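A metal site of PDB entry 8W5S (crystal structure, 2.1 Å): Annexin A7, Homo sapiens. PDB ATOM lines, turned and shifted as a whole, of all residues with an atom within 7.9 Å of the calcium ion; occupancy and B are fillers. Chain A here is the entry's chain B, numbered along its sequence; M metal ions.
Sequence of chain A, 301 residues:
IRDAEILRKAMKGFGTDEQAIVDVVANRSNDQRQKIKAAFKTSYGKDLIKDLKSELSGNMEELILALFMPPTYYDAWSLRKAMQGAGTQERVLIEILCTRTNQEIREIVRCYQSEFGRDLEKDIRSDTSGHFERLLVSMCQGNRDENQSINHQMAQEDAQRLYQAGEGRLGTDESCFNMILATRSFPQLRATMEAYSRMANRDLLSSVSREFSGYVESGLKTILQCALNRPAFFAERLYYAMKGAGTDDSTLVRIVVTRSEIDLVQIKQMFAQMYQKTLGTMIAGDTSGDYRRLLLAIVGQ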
ATOM      1  N   ARG A  80      11.826 -14.496 -14.657  1.00  0.00           N
ATOM      2  CA  ARG A  80      11.806 -13.296 -15.492  1.00  0.00           C
ATOM      3  C   ARG A  80      10.375 -12.822 -15.719  1.00  0.00           C
ATOM      4  O   ARG A  80      10.106 -11.621 -15.677  1.00  0.00           O
ATOM      5  CB  ARG A  80      12.502 -13.557 -16.821  1.00  0.00           C
ATOM      6  CG  ARG A  80      12.430 -12.353 -17.740  1.00  0.00           C
ATOM      7  CD  ARG A  80      13.335 -11.274 -17.169  1.00  0.00           C
ATOM      8  NE  ARG A  80      13.143  -9.957 -17.768  1.00  0.00           N
ATOM      9  CZ  ARG A  80      12.926  -8.854 -17.067  1.00  0.00           C
ATOM     10  NH1 ARG A  80      12.799  -8.883 -15.752  1.00  0.00           N
ATOM     11  NH2 ARG A  80      12.811  -7.693 -17.698  1.00  0.00           N
ATOM     12  N   LYS A  81       9.449 -13.762 -15.938  1.00  0.00           N
ATOM     13  CA  LYS A  81       8.045 -13.397 -16.112  1.00  0.00           C
ATOM     14  C   LYS A  81       7.492 -12.749 -14.846  1.00  0.00           C
ATOM     15  O   LYS A  81       6.681 -11.814 -14.920  1.00  0.00           O
ATOM     16  CB  LYS A  81       7.234 -14.640 -16.478  1.00  0.00           C
ATOM     17  CG  LYS A  81       5.755 -14.376 -16.733  1.00  0.00           C
ATOM     18  CD  LYS A  81       4.936 -15.625 -16.434  1.00  0.00           C
ATOM     19  CE  LYS A  81       3.783 -15.808 -17.414  1.00  0.00           C
ATOM     20  NZ  LYS A  81       3.003 -14.551 -17.630  1.00  0.00           N
ATOM     21  N   ALA A  82       7.914 -13.226 -13.668  1.00  0.00           N
ATOM     22  CA  ALA A  82       7.347 -12.761 -12.419  1.00  0.00           C
ATOM     23  C   ALA A  82       7.637 -11.290 -12.159  1.00  0.00           C
ATOM     24  O   ALA A  82       6.852 -10.611 -11.490  1.00  0.00           O
ATOM     25  CB  ALA A  82       7.865 -13.622 -11.262  1.00  0.00           C
ATOM     26  N   MET A  83       8.757 -10.779 -12.671  1.00  0.00           N
ATOM     27  CA  MET A  83       9.114  -9.377 -12.519  1.00  0.00           C
ATOM     28  C   MET A  83       8.894  -8.563 -13.781  1.00  0.00           C
ATOM     29  O   MET A  83       9.051  -7.329 -13.743  1.00  0.00           O
ATOM     30  CB  MET A  83      10.577  -9.250 -12.073  1.00  0.00           C
ATOM     31  CG  MET A  83      10.900 -10.045 -10.826  1.00  0.00           C
ATOM     32  SD  MET A  83      12.660 -10.036 -10.435  1.00  0.00           S
ATOM     33  CE  MET A  83      13.151 -11.651 -11.023  1.00  0.00           C
ATOM     34  N   GLN A  84       8.538  -9.207 -14.886  1.00  0.00           N
ATOM     35  CA  GLN A  84       8.386  -8.535 -16.171  1.00  0.00           C
ATOM     36  C   GLN A  84       7.353  -7.422 -16.093  1.00  0.00           C
ATOM     37  O   GLN A  84       6.285  -7.584 -15.497  1.00  0.00           O
ATOM     38  CB  GLN A  84       7.995  -9.555 -17.240  1.00  0.00           C
ATOM     39  CG  GLN A  84       8.765  -9.465 -18.538  1.00  0.00           C
ATOM     40  CD  GLN A  84       8.568 -10.686 -19.400  1.00  0.00           C
ATOM     41  OE1 GLN A  84       7.521 -11.320 -19.369  1.00  0.00           O
ATOM     42  NE2 GLN A  84       9.593 -11.028 -20.183  1.00  0.00           N
ATOM     43  N   GLY A  85       7.671  -6.286 -16.717  1.00  0.00           N
ATOM     44  CA  GLY A  85       6.792  -5.133 -16.683  1.00  0.00           C
ATOM     45  C   GLY A  85       6.654  -4.534 -15.301  1.00  0.00           C
ATOM     46  O   GLY A  85       7.168  -5.100 -14.332  1.00  0.00           O
ATOM     47  N   ALA A  86       5.978  -3.396 -15.201  1.00  0.00           N
ATOM     48  CA  ALA A  86       5.685  -2.840 -13.889  1.00  0.00           C
ATOM     49  C   ALA A  86       4.876  -3.835 -13.069  1.00  0.00           C
ATOM     50  O   ALA A  86       4.157  -4.679 -13.611  1.00  0.00           O
ATOM     51  CB  ALA A  86       4.943  -1.516 -14.023  1.00  0.00           C
ATOM     52  N   GLY A  87       5.018  -3.751 -11.748  1.00  0.00           N
ATOM     53  CA  GLY A  87       4.387  -4.717 -10.876  1.00  0.00           C
ATOM     54  C   GLY A  87       5.159  -6.025 -10.835  1.00  0.00           C
ATOM     55  O   GLY A  87       6.171  -6.221 -11.503  1.00  0.00           O
ATOM     56  N   THR A  88       4.649  -6.950 -10.018  1.00  0.00           N
ATOM     57  CA  THR A  88       5.373  -8.192  -9.759  1.00  0.00           C
ATOM     58  C   THR A  88       4.404  -9.311  -9.411  1.00  0.00           C
ATOM     59  O   THR A  88       3.336  -9.076  -8.832  1.00  0.00           O
ATOM     60  CB  THR A  88       6.374  -8.018  -8.601  1.00  0.00           C
ATOM     61  OG1 THR A  88       6.915  -6.694  -8.620  1.00  0.00           O
ATOM     62  CG2 THR A  88       7.506  -9.019  -8.731  1.00  0.00           C
ATOM     63  N   GLN A  89       4.790 -10.533  -9.792  1.00  0.00           N
ATOM     64  CA  GLN A  89       4.143 -11.750  -9.285  1.00  0.00           C
ATOM     65  C   GLN A  89       4.958 -12.223  -8.088  1.00  0.00           C
ATOM     66  O   GLN A  89       5.816 -13.105  -8.182  1.00  0.00           O
ATOM     67  CB  GLN A  89       4.068 -12.819 -10.368  1.00  0.00           C
ATOM     68  CG  GLN A  89       3.274 -12.445 -11.604  1.00  0.00           C
ATOM     69  CD  GLN A  89       3.303 -13.539 -12.650  1.00  0.00           C
ATOM     70  OE1 GLN A  89       3.971 -14.565 -12.481  1.00  0.00           O
ATOM     71  NE2 GLN A  89       2.575 -13.340 -13.750  1.00  0.00           N
ATOM     72  N   ASP A 123      17.586  -7.649 -10.800  1.00  0.00           N
ATOM     73  CA  ASP A 123      16.201  -7.475 -11.211  1.00  0.00           C
ATOM     74  C   ASP A 123      15.247  -7.572 -10.022  1.00  0.00           C
ATOM     75  O   ASP A 123      14.226  -6.883  -9.992  1.00  0.00           O
ATOM     76  CB  ASP A 123      15.830  -8.532 -12.253  1.00  0.00           C
ATOM     77  CG  ASP A 123      16.545  -8.312 -13.573  1.00  0.00           C
ATOM     78  OD1 ASP A 123      17.177  -7.247 -13.737  1.00  0.00           O
ATOM     79  OD2 ASP A 123      16.487  -9.212 -14.437  1.00  0.00           O
ATOM     80  N   SER A 126      15.168  -4.207  -7.962  1.00  0.00           N
ATOM     81  CA  SER A 126      14.369  -3.150  -8.564  1.00  0.00           C
ATOM     82  C   SER A 126      12.897  -3.499  -8.676  1.00  0.00           C
ATOM     83  O   SER A 126      12.078  -2.615  -8.942  1.00  0.00           O
ATOM     84  CB  SER A 126      14.929  -2.811  -9.956  1.00  0.00           C
ATOM     85  OG  SER A 126      14.944  -3.947 -10.789  1.00  0.00           O
ATOM     86  N   ASP A 127      12.520  -4.763  -8.476  1.00  0.00           N
ATOM     87  CA  ASP A 127      11.119  -5.165  -8.528  1.00  0.00           C
ATOM     88  C   ASP A 127      10.489  -5.347  -7.146  1.00  0.00           C
ATOM     89  O   ASP A 127       9.265  -5.256  -7.034  1.00  0.00           O
ATOM     90  CB  ASP A 127      10.960  -6.468  -9.325  1.00  0.00           C
ATOM     91  CG  ASP A 127      10.096  -6.276 -10.553  1.00  0.00           C
ATOM     92  OD1 ASP A 127      10.590  -5.713 -11.554  1.00  0.00           O
ATOM     93  OD2 ASP A 127       8.918  -6.700 -10.528  1.00  0.00           O
ATOM     94  N   THR A 128      11.286  -5.617  -6.121  1.00  0.00           N
ATOM     95  CA  THR A 128      10.807  -5.766  -4.755  1.00  0.00           C
ATOM     96  C   THR A 128      11.511  -4.749  -3.854  1.00  0.00           C
ATOM     97  O   THR A 128      12.435  -4.051  -4.277  1.00  0.00           O
ATOM     98  CB  THR A 128      11.051  -7.196  -4.236  1.00  0.00           C
ATOM     99  OG1 THR A 128      12.454  -7.445  -4.145  1.00  0.00           O
ATOM    100  CG2 THR A 128      10.415  -8.206  -5.179  1.00  0.00           C
HETATM  101 CA    CA M   1       8.271  -5.399 -12.562  1.00  0.00          CA
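O of Asp 127 is in hydrogen-bond range of OG1 of Thr 88, at 3.2 Å.
Merely in contact with the calcium ion: Ala 86 (3.8 Å).
The calcium ion is bound by O of Gly 85 (2.1 Å), O of Met 83 (2.4 Å), O of Gly 87 (2.5 Å), OD2 of Asp 127 (2.5 Å) and OD1 of Asp 127 (2.5 Å). The calcium ion has five donor atoms within binding distance.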
